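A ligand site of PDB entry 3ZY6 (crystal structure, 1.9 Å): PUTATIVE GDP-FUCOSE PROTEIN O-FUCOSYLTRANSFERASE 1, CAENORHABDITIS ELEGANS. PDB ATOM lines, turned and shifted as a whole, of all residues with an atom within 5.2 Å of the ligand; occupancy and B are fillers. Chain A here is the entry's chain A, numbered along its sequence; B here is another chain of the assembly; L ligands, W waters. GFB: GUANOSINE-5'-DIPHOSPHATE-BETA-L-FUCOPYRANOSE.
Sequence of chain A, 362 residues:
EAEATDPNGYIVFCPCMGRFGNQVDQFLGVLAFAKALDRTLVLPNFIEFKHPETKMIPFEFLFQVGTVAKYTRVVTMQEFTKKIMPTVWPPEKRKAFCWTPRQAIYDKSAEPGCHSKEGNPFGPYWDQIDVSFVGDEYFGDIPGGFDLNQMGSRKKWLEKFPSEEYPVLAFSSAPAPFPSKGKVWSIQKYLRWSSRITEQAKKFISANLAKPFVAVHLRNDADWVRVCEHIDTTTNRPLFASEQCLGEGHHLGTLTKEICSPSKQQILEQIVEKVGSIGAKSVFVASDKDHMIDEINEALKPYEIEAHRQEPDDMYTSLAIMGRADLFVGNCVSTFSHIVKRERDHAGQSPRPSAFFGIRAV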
ATOM      1  N   GLY A  18       2.527  30.145 -10.113  1.00  0.00           N
ATOM      2  CA  GLY A  18       1.229  29.499 -10.022  1.00  0.00           C
ATOM      3  C   GLY A  18       1.230  28.021 -10.417  1.00  0.00           C
ATOM      4  O   GLY A  18       2.264  27.462 -10.739  1.00  0.00           O
ATOM      5  N   ARG A  19       0.051  27.427 -10.391  1.00  0.00           N
ATOM      6  CA  ARG A  19      -0.125  26.055 -10.779  1.00  0.00           C
ATOM      7  C   ARG A  19      -0.340  25.866 -12.280  1.00  0.00           C
ATOM      8  O   ARG A  19      -0.176  26.824 -13.049  1.00  0.00           O
ATOM      9  CB  ARG A  19      -1.223  25.473  -9.928  1.00  0.00           C
ATOM     10  CG  ARG A  19      -0.646  25.204  -8.534  1.00  0.00           C
ATOM     11  CD  ARG A  19      -1.683  24.743  -7.598  1.00  0.00           C
ATOM     12  NE  ARG A  19      -2.531  25.842  -7.139  1.00  0.00           N
ATOM     13  CZ  ARG A  19      -3.621  25.681  -6.413  1.00  0.00           C
ATOM     14  NH1 ARG A  19      -3.995  24.443  -6.069  1.00  0.00           N
ATOM     15  NH2 ARG A  19      -4.330  26.731  -6.025  1.00  0.00           N
ATOM     16  N   PHE A  20      -0.666  24.643 -12.712  1.00  0.00           N
ATOM     17  CA  PHE A  20      -0.670  24.347 -14.168  1.00  0.00           C
ATOM     18  C   PHE A  20      -1.382  25.395 -15.067  1.00  0.00           C
ATOM     19  O   PHE A  20      -0.853  25.802 -16.133  1.00  0.00           O
ATOM     20  CB  PHE A  20      -1.253  22.954 -14.399  1.00  0.00           C
ATOM     21  CG  PHE A  20      -1.005  22.416 -15.759  1.00  0.00           C
ATOM     22  CD1 PHE A  20       0.294  22.318 -16.270  1.00  0.00           C
ATOM     23  CD2 PHE A  20      -2.069  22.027 -16.561  1.00  0.00           C
ATOM     24  CE1 PHE A  20       0.517  21.803 -17.563  1.00  0.00           C
ATOM     25  CE2 PHE A  20      -1.861  21.524 -17.843  1.00  0.00           C
ATOM     26  CZ  PHE A  20      -0.550  21.422 -18.360  1.00  0.00           C
ATOM     27  N   GLY A  21      -2.570  25.811 -14.670  1.00  0.00           N
ATOM     28  CA  GLY A  21      -3.302  26.833 -15.427  1.00  0.00           C
ATOM     29  C   GLY A  21      -2.494  28.101 -15.617  1.00  0.00           C
ATOM     30  O   GLY A  21      -2.460  28.657 -16.725  1.00  0.00           O
ATOM     31  N   ASN A  22      -1.858  28.586 -14.547  1.00  0.00           N
ATOM     32  CA  ASN A  22      -1.003  29.806 -14.645  1.00  0.00           C
ATOM     33  C   ASN A  22       0.206  29.520 -15.539  1.00  0.00           C
ATOM     34  O   ASN A  22       0.574  30.348 -16.360  1.00  0.00           O
ATOM     35  CB  ASN A  22      -0.485  30.263 -13.270  1.00  0.00           C
ATOM     36  CG  ASN A  22      -1.557  30.926 -12.400  1.00  0.00           C
ATOM     37  OD1 ASN A  22      -1.230  31.667 -11.454  1.00  0.00           O
ATOM     38  ND2 ASN A  22      -2.838  30.678 -12.712  1.00  0.00           N
ATOM     39  N   HIS A 217     -16.271  21.765 -14.731  1.00  0.00           N
ATOM     40  CA  HIS A 217     -15.169  22.033 -13.844  1.00  0.00           C
ATOM     41  C   HIS A 217     -15.683  22.688 -12.547  1.00  0.00           C
ATOM     42  O   HIS A 217     -16.266  23.770 -12.560  1.00  0.00           O
ATOM     43  CB  HIS A 217     -14.045  22.822 -14.549  1.00  0.00           C
ATOM     44  CG  HIS A 217     -12.895  23.145 -13.651  1.00  0.00           C
ATOM     45  ND1 HIS A 217     -12.267  24.368 -13.628  1.00  0.00           N
ATOM     46  CD2 HIS A 217     -12.279  22.386 -12.708  1.00  0.00           C
ATOM     47  CE1 HIS A 217     -11.308  24.351 -12.707  1.00  0.00           C
ATOM     48  NE2 HIS A 217     -11.293  23.162 -12.129  1.00  0.00           N
ATOM     49  N   LEU A 218     -15.498  21.994 -11.439  1.00  0.00           N
ATOM     50  CA  LEU A 218     -15.965  22.489 -10.143  1.00  0.00           C
ATOM     51  C   LEU A 218     -14.747  22.852  -9.330  1.00  0.00           C
ATOM     52  O   LEU A 218     -14.057  21.985  -8.803  1.00  0.00           O
ATOM     53  CB  LEU A 218     -16.778  21.429  -9.419  1.00  0.00           C
ATOM     54  CG  LEU A 218     -18.028  20.868 -10.097  1.00  0.00           C
ATOM     55  CD1 LEU A 218     -18.724  19.896  -9.105  1.00  0.00           C
ATOM     56  CD2 LEU A 218     -18.980  22.025 -10.558  1.00  0.00           C
ATOM     57  N   ARG A 219     -14.453  24.150  -9.262  1.00  0.00           N
ATOM     58  CA  ARG A 219     -13.264  24.607  -8.528  1.00  0.00           C
ATOM     59  C   ARG A 219     -13.811  25.097  -7.183  1.00  0.00           C
ATOM     60  O   ARG A 219     -14.519  26.114  -7.114  1.00  0.00           O
ATOM     61  CB  ARG A 219     -12.534  25.691  -9.340  1.00  0.00           C
ATOM     62  CG  ARG A 219     -11.297  26.297  -8.679  1.00  0.00           C
ATOM     63  CD  ARG A 219      -9.994  25.510  -8.899  1.00  0.00           C
ATOM     64  NE  ARG A 219      -8.830  26.362  -8.597  1.00  0.00           N
ATOM     65  CZ  ARG A 219      -8.229  26.447  -7.407  1.00  0.00           C
ATOM     66  NH1 ARG A 219      -8.645  25.695  -6.387  1.00  0.00           N
ATOM     67  NH2 ARG A 219      -7.204  27.264  -7.240  1.00  0.00           N
ATOM     68  N   ASP A 223      -8.879  27.551  -0.431  1.00  0.00           N
ATOM     69  CA  ASP A 223      -8.106  28.694  -0.965  1.00  0.00           C
ATOM     70  C   ASP A 223      -8.904  29.452  -2.037  1.00  0.00           C
ATOM     71  O   ASP A 223      -8.840  30.668  -2.126  1.00  0.00           O
ATOM     72  CB  ASP A 223      -6.741  28.231  -1.512  1.00  0.00           C
ATOM     73  CG  ASP A 223      -5.781  27.774  -0.396  1.00  0.00           C
ATOM     74  OD1 ASP A 223      -6.086  27.995   0.804  1.00  0.00           O
ATOM     75  OD2 ASP A 223      -4.725  27.175  -0.723  1.00  0.00           O
ATOM     76  N   TRP A 224      -9.682  28.700  -2.824  1.00  0.00           N
ATOM     77  CA  TRP A 224     -10.514  29.297  -3.856  1.00  0.00           C
ATOM     78  C   TRP A 224     -11.662  30.121  -3.276  1.00  0.00           C
ATOM     79  O   TRP A 224     -11.893  31.241  -3.732  1.00  0.00           O
ATOM     80  CB  TRP A 224     -11.061  28.210  -4.766  1.00  0.00           C
ATOM     81  CG  TRP A 224     -11.748  28.727  -5.949  1.00  0.00           C
ATOM     82  CD1 TRP A 224     -13.095  28.818  -6.147  1.00  0.00           C
ATOM     83  CD2 TRP A 224     -11.130  29.280  -7.122  1.00  0.00           C
ATOM     84  NE1 TRP A 224     -13.356  29.368  -7.387  1.00  0.00           N
ATOM     85  CE2 TRP A 224     -12.163  29.652  -8.012  1.00  0.00           C
ATOM     86  CE3 TRP A 224      -9.791  29.477  -7.521  1.00  0.00           C
ATOM     87  CZ2 TRP A 224     -11.918  30.222  -9.274  1.00  0.00           C
ATOM     88  CZ3 TRP A 224      -9.542  30.031  -8.794  1.00  0.00           C
ATOM     89  CH2 TRP A 224     -10.614  30.400  -9.642  1.00  0.00           C
ATOM     90  N   VAL A 227     -10.259  33.351  -2.292  1.00  0.00           N
ATOM     91  CA  VAL A 227      -9.971  34.246  -3.412  1.00  0.00           C
ATOM     92  C   VAL A 227     -11.256  34.904  -3.930  1.00  0.00           C
ATOM     93  O   VAL A 227     -11.301  36.124  -4.126  1.00  0.00           O
ATOM     94  CB  VAL A 227      -9.139  33.559  -4.509  1.00  0.00           C
ATOM     95  CG1 VAL A 227      -8.946  34.483  -5.711  1.00  0.00           C
ATOM     96  CG2 VAL A 227      -7.788  33.138  -3.966  1.00  0.00           C
ATOM     97  N   PHE A 240      -7.483  36.493 -12.436  1.00  0.00           N
ATOM     98  CA  PHE A 240      -7.015  35.311 -13.152  1.00  0.00           C
ATOM     99  C   PHE A 240      -7.650  35.283 -14.550  1.00  0.00           C
ATOM    100  O   PHE A 240      -7.466  36.242 -15.311  1.00  0.00           O
ATOM    101  CB  PHE A 240      -7.261  34.078 -12.284  1.00  0.00           C
ATOM    102  CG  PHE A 240      -6.599  34.184 -10.952  1.00  0.00           C
ATOM    103  CD1 PHE A 240      -5.217  34.281 -10.872  1.00  0.00           C
ATOM    104  CD2 PHE A 240      -7.348  34.249  -9.777  1.00  0.00           C
ATOM    105  CE1 PHE A 240      -4.576  34.417  -9.612  1.00  0.00           C
ATOM    106  CE2 PHE A 240      -6.728  34.384  -8.525  1.00  0.00           C
ATOM    107  CZ  PHE A 240      -5.344  34.476  -8.437  1.00  0.00           C
ATOM    108  N   ALA A 286     -14.870  17.269 -13.183  1.00  0.00           N
ATOM    109  CA  ALA A 286     -13.507  17.496 -12.770  1.00  0.00           C
ATOM    110  C   ALA A 286     -13.540  18.486 -11.607  1.00  0.00           C
ATOM    111  O   ALA A 286     -14.171  19.544 -11.695  1.00  0.00           O
ATOM    112  CB  ALA A 286     -12.709  18.042 -13.913  1.00  0.00           C
ATOM    113  N   SER A 287     -12.884  18.135 -10.518  1.00  0.00           N
ATOM    114  CA  SER A 287     -12.866  18.987  -9.331  1.00  0.00           C
ATOM    115  C   SER A 287     -11.519  18.943  -8.651  1.00  0.00           C
ATOM    116  O   SER A 287     -10.846  17.908  -8.653  1.00  0.00           O
ATOM    117  CB  SER A 287     -13.940  18.550  -8.337  1.00  0.00           C
ATOM    118  OG  SER A 287     -14.183  19.591  -7.409  1.00  0.00           O
ATOM    119  N   ASP A 288     -11.150  20.075  -8.046  1.00  0.00           N
ATOM    120  CA  ASP A 288      -9.998  20.141  -7.151  1.00  0.00           C
ATOM    121  C   ASP A 288     -10.280  19.604  -5.752  1.00  0.00           C
ATOM    122  O   ASP A 288      -9.355  19.407  -4.983  1.00  0.00           O
ATOM    123  CB  ASP A 288      -9.495  21.586  -7.013  1.00  0.00           C
ATOM    124  CG  ASP A 288     -10.596  22.559  -6.507  1.00  0.00           C
ATOM    125  OD1 ASP A 288     -11.795  22.264  -6.639  1.00  0.00           O
ATOM    126  OD2 ASP A 288     -10.226  23.612  -5.951  1.00  0.00           O
ATOM    127  N   ASP A 313      -8.567  11.844  -9.265  1.00  0.00           N
ATOM    128  CA  ASP A 313      -8.762  12.819 -10.354  1.00  0.00           C
ATOM    129  C   ASP A 313      -7.393  13.257 -10.897  1.00  0.00           C
ATOM    130  O   ASP A 313      -6.666  13.963 -10.211  1.00  0.00           O
ATOM    131  CB  ASP A 313      -9.604  14.013  -9.850  1.00  0.00           C
ATOM    132  CG  ASP A 313     -10.049  14.947 -10.983  1.00  0.00           C
ATOM    133  OD1 ASP A 313      -9.242  15.169 -11.898  1.00  0.00           O
ATOM    134  OD2 ASP A 313     -11.211  15.418 -10.951  1.00  0.00           O
ATOM    135  N   ASP A 314      -7.062  12.803 -12.127  1.00  0.00           N
ATOM    136  CA  ASP A 314      -5.806  13.185 -12.800  1.00  0.00           C
ATOM    137  C   ASP A 314      -6.070  14.460 -13.535  1.00  0.00           C
ATOM    138  O   ASP A 314      -6.940  14.498 -14.414  1.00  0.00           O
ATOM    139  CB  ASP A 314      -5.360  12.152 -13.837  1.00  0.00           C
ATOM    140  CG  ASP A 314      -3.985  12.462 -14.389  1.00  0.00           C
ATOM    141  OD1 ASP A 314      -3.008  12.155 -13.673  1.00  0.00           O
ATOM    142  OD2 ASP A 314      -3.851  13.030 -15.510  1.00  0.00           O
ATOM    143  N   MET A 315      -5.331  15.515 -13.198  1.00  0.00           N
ATOM    144  CA  MET A 315      -5.704  16.824 -13.735  1.00  0.00           C
ATOM    145  C   MET A 315      -5.519  16.907 -15.236  1.00  0.00           C
ATOM    146  O   MET A 315      -6.224  17.672 -15.894  1.00  0.00           O
ATOM    147  CB  MET A 315      -4.937  17.959 -13.044  1.00  0.00           C
ATOM    148  CG  MET A 315      -3.518  18.192 -13.556  1.00  0.00           C
ATOM    149  SD  MET A 315      -2.605  19.422 -12.577  1.00  0.00           S
ATOM    150  CE  MET A 315      -2.138  18.433 -11.207  1.00  0.00           C
ATOM    151  N   SER A 318      -8.240  14.842 -16.993  1.00  0.00           N
ATOM    152  CA  SER A 318      -9.463  15.635 -16.822  1.00  0.00           C
ATOM    153  C   SER A 318      -9.577  16.768 -17.819  1.00  0.00           C
ATOM    154  O   SER A 318     -10.620  16.920 -18.460  1.00  0.00           O
ATOM    155  CB  SER A 318      -9.583  16.203 -15.399  1.00  0.00           C
ATOM    156  OG  SER A 318      -9.912  15.145 -14.514  1.00  0.00           O
ATOM    157  N   MET A 322     -12.490  17.060 -20.807  1.00  0.00           N
ATOM    158  CA  MET A 322     -13.333  18.234 -20.935  1.00  0.00           C
ATOM    159  C   MET A 322     -13.161  18.862 -22.313  1.00  0.00           C
ATOM    160  O   MET A 322     -14.106  19.461 -22.880  1.00  0.00           O
ATOM    161  CB  MET A 322     -13.021  19.251 -19.816  1.00  0.00           C
ATOM    162  CG  MET A 322     -13.322  18.671 -18.416  1.00  0.00           C
ATOM    163  SD  MET A 322     -13.243  19.897 -17.097  1.00  0.00           S
ATOM    164  CE  MET A 322     -11.468  19.945 -16.891  1.00  0.00           C
ATOM    165  N   VAL A 333     -13.385  32.160 -13.594  1.00  0.00           N
ATOM    166  CA  VAL A 333     -12.179  32.724 -12.976  1.00  0.00           C
ATOM    167  C   VAL A 333     -10.934  31.826 -13.110  1.00  0.00           C
ATOM    168  O   VAL A 333      -9.804  32.311 -13.049  1.00  0.00           O
ATOM    169  CB  VAL A 333     -12.441  33.106 -11.519  1.00  0.00           C
ATOM    170  CG1 VAL A 333     -11.194  33.779 -10.879  1.00  0.00           C
ATOM    171  CG2 VAL A 333     -13.656  34.036 -11.456  1.00  0.00           C
ATOM    172  N   SER A 334     -11.159  30.533 -13.248  1.00  0.00           N
ATOM    173  CA  SER A 334     -10.087  29.562 -13.235  1.00  0.00           C
ATOM    174  C   SER A 334      -9.317  29.556 -14.544  1.00  0.00           C
ATOM    175  O   SER A 334      -9.891  29.321 -15.592  1.00  0.00           O
ATOM    176  CB  SER A 334     -10.642  28.155 -12.992  1.00  0.00           C
ATOM    177  OG  SER A 334      -9.567  27.211 -12.963  1.00  0.00           O
ATOM    178  N   THR A 335      -8.008  29.762 -14.454  1.00  0.00           N
ATOM    179  CA  THR A 335      -7.078  29.511 -15.589  1.00  0.00           C
ATOM    180  C   THR A 335      -7.040  28.014 -16.015  1.00  0.00           C
ATOM    181  O   THR A 335      -6.612  27.670 -17.091  1.00  0.00           O
ATOM    182  CB  THR A 335      -5.616  29.963 -15.249  1.00  0.00           C
ATOM    183  OG1 THR A 335      -5.102  29.176 -14.160  1.00  0.00           O
ATOM    184  CG2 THR A 335      -5.556  31.477 -14.882  1.00  0.00           C
ATOM    185  N   PHE A 336      -7.498  27.144 -15.131  1.00  0.00           N
ATOM    186  CA  PHE A 336      -7.590  25.740 -15.436  1.00  0.00           C
ATOM    187  C   PHE A 336      -8.740  25.517 -16.428  1.00  0.00           C
ATOM    188  O   PHE A 336      -8.552  24.927 -17.497  1.00  0.00           O
ATOM    189  CB  PHE A 336      -7.788  24.981 -14.132  1.00  0.00           C
ATOM    190  CG  PHE A 336      -7.637  23.485 -14.236  1.00  0.00           C
ATOM    191  CD1 PHE A 336      -6.382  22.888 -14.150  1.00  0.00           C
ATOM    192  CD2 PHE A 336      -8.774  22.664 -14.370  1.00  0.00           C
ATOM    193  CE1 PHE A 336      -6.250  21.490 -14.225  1.00  0.00           C
ATOM    194  CE2 PHE A 336      -8.648  21.250 -14.441  1.00  0.00           C
ATOM    195  CZ  PHE A 336      -7.391  20.680 -14.376  1.00  0.00           C
ATOM    196  N   GLU B 111      -1.289  33.575  -2.761  1.00  0.00           N
ATOM    197  CA  GLU B 111      -1.981  34.000  -3.976  1.00  0.00           C
ATOM    198  C   GLU B 111      -1.153  35.041  -4.739  1.00  0.00           C
ATOM    199  O   GLU B 111      -0.609  35.970  -4.128  1.00  0.00           O
ATOM    200  CB  GLU B 111      -3.348  34.625  -3.652  1.00  0.00           C
ATOM    201  CG  GLU B 111      -4.075  34.060  -2.415  1.00  0.00           C
ATOM    202  CD  GLU B 111      -5.226  34.954  -1.959  1.00  0.00           C
ATOM    203  OE1 GLU B 111      -5.304  36.120  -2.419  1.00  0.00           O
ATOM    204  OE2 GLU B 111      -6.058  34.492  -1.139  1.00  0.00           O
ATOM    205  N   PRO B 112      -1.066  34.904  -6.081  1.00  0.00           N
ATOM    206  CA  PRO B 112      -0.312  35.873  -6.896  1.00  0.00           C
ATOM    207  C   PRO B 112      -0.829  37.310  -6.728  1.00  0.00           C
ATOM    208  O   PRO B 112      -2.012  37.582  -6.980  1.00  0.00           O
ATOM    209  CB  PRO B 112      -0.530  35.389  -8.327  1.00  0.00           C
ATOM    210  CG  PRO B 112      -0.867  33.938  -8.205  1.00  0.00           C
ATOM    211  CD  PRO B 112      -1.617  33.805  -6.902  1.00  0.00           C
HETATM  212  O1P GFB L   1      -4.298  25.221 -12.524  1.00  0.00           O
HETATM  213  P   GFB L   1      -4.317  26.514 -11.751  1.00  0.00           P
HETATM  214  O3P GFB L   1      -3.178  27.505 -11.978  1.00  0.00           O
HETATM  215  O2P GFB L   1      -5.768  27.151 -12.068  1.00  0.00           O
HETATM  216  O5' GFB L   1      -4.381  26.135 -10.182  1.00  0.00           O
HETATM  217  P1  GFB L   1      -6.607  28.258 -11.249  1.00  0.00           P
HETATM  218  C5' GFB L   1      -5.365  25.202  -9.773  1.00  0.00           C
HETATM  219  C4' GFB L   1      -4.698  23.861  -9.508  1.00  0.00           C
HETATM  220  O4' GFB L   1      -5.505  23.147  -8.597  1.00  0.00           O
HETATM  221  C3' GFB L   1      -4.624  22.972 -10.749  1.00  0.00           C
HETATM  222  C1' GFB L   1      -5.757  21.813  -9.053  1.00  0.00           C
HETATM  223  O3' GFB L   1      -3.416  23.157 -11.497  1.00  0.00           O
HETATM  224  C2' GFB L   1      -4.709  21.595 -10.134  1.00  0.00           C
HETATM  225  O2' GFB L   1      -3.459  21.238  -9.543  1.00  0.00           O
HETATM  226  N9  GFB L   1      -7.080  21.675  -9.730  1.00  0.00           N
HETATM  227  C8  GFB L   1      -7.960  22.632 -10.102  1.00  0.00           C
HETATM  228  C4  GFB L   1      -7.538  20.509 -10.135  1.00  0.00           C
HETATM  229  N7  GFB L   1      -9.007  22.063 -10.721  1.00  0.00           N
HETATM  230  C5  GFB L   1      -8.746  20.725 -10.774  1.00  0.00           C
HETATM  231  C6  GFB L   1      -9.423  19.622 -11.273  1.00  0.00           C
HETATM  232  O6  GFB L   1     -10.525  19.766 -11.835  1.00  0.00           O
HETATM  233  N1  GFB L   1      -8.894  18.384 -11.107  1.00  0.00           N
HETATM  234  C2  GFB L   1      -7.706  18.199 -10.504  1.00  0.00           C
HETATM  235  N2  GFB L   1      -7.167  16.963 -10.374  1.00  0.00           N
HETATM  236  N3  GFB L   1      -7.033  19.246 -10.015  1.00  0.00           N
HETATM  237  C1  GFB L   1      -5.308  29.607  -9.347  1.00  0.00           C
HETATM  238  C2A GFB L   1      -3.817  29.496  -9.096  1.00  0.00           C
HETATM  239  O1  GFB L   1      -5.765  28.360  -9.873  1.00  0.00           O
HETATM  240  O5  GFB L   1      -5.956  29.865  -8.087  1.00  0.00           O
HETATM  241  C3  GFB L   1      -3.269  30.793  -8.499  1.00  0.00           C
HETATM  242  O2  GFB L   1      -3.056  29.044 -10.224  1.00  0.00           O
HETATM  243  C4A GFB L   1      -3.917  30.888  -7.124  1.00  0.00           C
HETATM  244  O3  GFB L   1      -1.832  30.742  -8.414  1.00  0.00           O
HETATM  245  C5A GFB L   1      -5.441  30.916  -7.229  1.00  0.00           C
HETATM  246  O4  GFB L   1      -3.532  29.737  -6.338  1.00  0.00           O
HETATM  247  C6A GFB L   1      -6.071  30.808  -5.840  1.00  0.00           C
HETATM  248  O1X GFB L   1      -6.493  29.555 -12.026  1.00  0.00           O
HETATM  249  O2X GFB L   1      -7.928  27.599 -10.983  1.00  0.00           O
HETATM  250  O   HOH W   1      -1.333  28.199  -7.553  1.00  0.00           O
HETATM  251  O   HOH W   2      -4.600  16.218  -9.321  1.00  0.00           O
HETATM  252  O   HOH W   3      -2.273  21.938  -6.633  1.00  0.00           O
HETATM  253  O   HOH W   4      -0.790  22.322 -10.820  1.00  0.00           O
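OD1 of Asp 313 lies within hydrogen-bond range of N2 of the ligand (3.1 Å).
O2' of the ligand sits close to SD of Met 315 (3.6 Å).
The guanidinium group (NE) of Arg 219 is in salt-bridge range of an oxygen (O2X) of the ligand, at 2.8 Å.
An oxygen (O2) of the ligand is in hydrogen-bond range of the side-chain amide nitrogen of Asn 22.
O1P of the ligand sits at hydrogen-bond distance from N of Gly 21 (2.8 Å).
The backbone NH (N) of Ser 287 is in hydrogen-bond range of an oxygen (O6) of the ligand, at 3.2 Å.
NE2 of His 217 lies within hydrogen-bond range of N7 of the ligand (2.9 Å).
N1 of the ligand is in hydrogen-bond range of O of Ser 287, at 3.2 Å.
N of Thr 335 sits at hydrogen-bond distance from O1X of the ligand, at 2.9 Å.
The backbone NH (N) of Asn 22 lies within hydrogen-bond range of an oxygen (O3P) of the ligand (3.1 Å).
O4 of the ligand sits at hydrogen-bond distance from NH2 of Arg 19, 3.1 Å away.
O1X of the ligand sits at hydrogen-bond distance from OG1 of Thr 335 (2.6 Å).
A nitrogen (N2) of the ligand is in hydrogen-bond range of the backbone carbonyl oxygen of Asp 313, 3.0 Å away.
O2X of the ligand sits at hydrogen-bond distance from OG of Ser 334 (2.6 Å).
O3' of the ligand is in hydrogen-bond range of N of Phe 20 (3.4 Å).
OG of Ser 318 lies within hydrogen-bond range of OD1 of Asp 313 (2.7 Å).
The side-chain carboxylate (OD2) of Asp 288 is in salt-bridge range of the guanidinium group (NH1) of Arg 219 (2.7 Å).
N of Phe 336 sits at hydrogen-bond distance from OG of Ser 334.
The backbone carbonyl oxygen of Arg 219 lies close to the indole nitrogen of Trp 224.
The backbone carbonyl oxygen (O) of Leu 218 is in hydrogen-bond range of the side-chain hydroxyl (OG) of Ser 287.
The side-chain hydroxyl of Thr 335 lies within hydrogen-bond range of the side-chain amide nitrogen of Asn 22.
OD2 of Asp 313 is in hydrogen-bond range of N of Ser 287, 3.2 Å away.
The backbone carbonyl oxygen (O) of Ala 286 sits at hydrogen-bond distance from the backbone NH (N) of Leu 218.
CA of Gly 18 touches O3 of the ligand (3.7 Å).
Trp 224 touches the ligand.
Val 227 touches the ligand (CG2 to C6A, 3.4 Å).
CZ of Phe 240 touches C5A of the ligand, 3.8 Å away.
Ala 286 touches the ligand (C to O6, 3.3 Å).
Asp 288 touches the ligand.
Phe 336 touches the ligand.
CG of Pro 112 of chain B touches O3 of the ligand, 3.3 Å away.
Hydrophobic or aromatic side chains within 4 Å of the ligand: Phe 20, His 217, Trp 224, Val 227, Phe 240, Ala 286, Met 315, Phe 336 and Pro 112 of chain B.
19 residues have an atom within 4 Å of the ligand: Gly 18, Arg 19, Phe 20, Gly 21, Asn 22, His 217, Arg 219, Trp 224, Val 227, Phe 240, Ala 286, Ser 287, Asp 288, Asp 313, Met 315, Ser 334, Thr 335, Phe 336 and Pro 112 of chain B.
The nearest printed residue that does not touch the ligand is Asp 314 (4.2 Å).
Water W1 bridges the guanidinium group (NE) of Arg 19 (2.7 Å) and an oxygen (O3) of the ligand (2.7 Å).
Water W4 bridges O3' of the ligand and N of Phe 20.
Water W2 lies within hydrogen-bond range of a nitrogen (N2) of the ligand and the backbone carbonyl oxygen (O) of Asp 313.
Water W3 lies within hydrogen-bond range of NH1 of Arg 19 (3.1 Å) and O2' of the ligand (3.2 Å).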
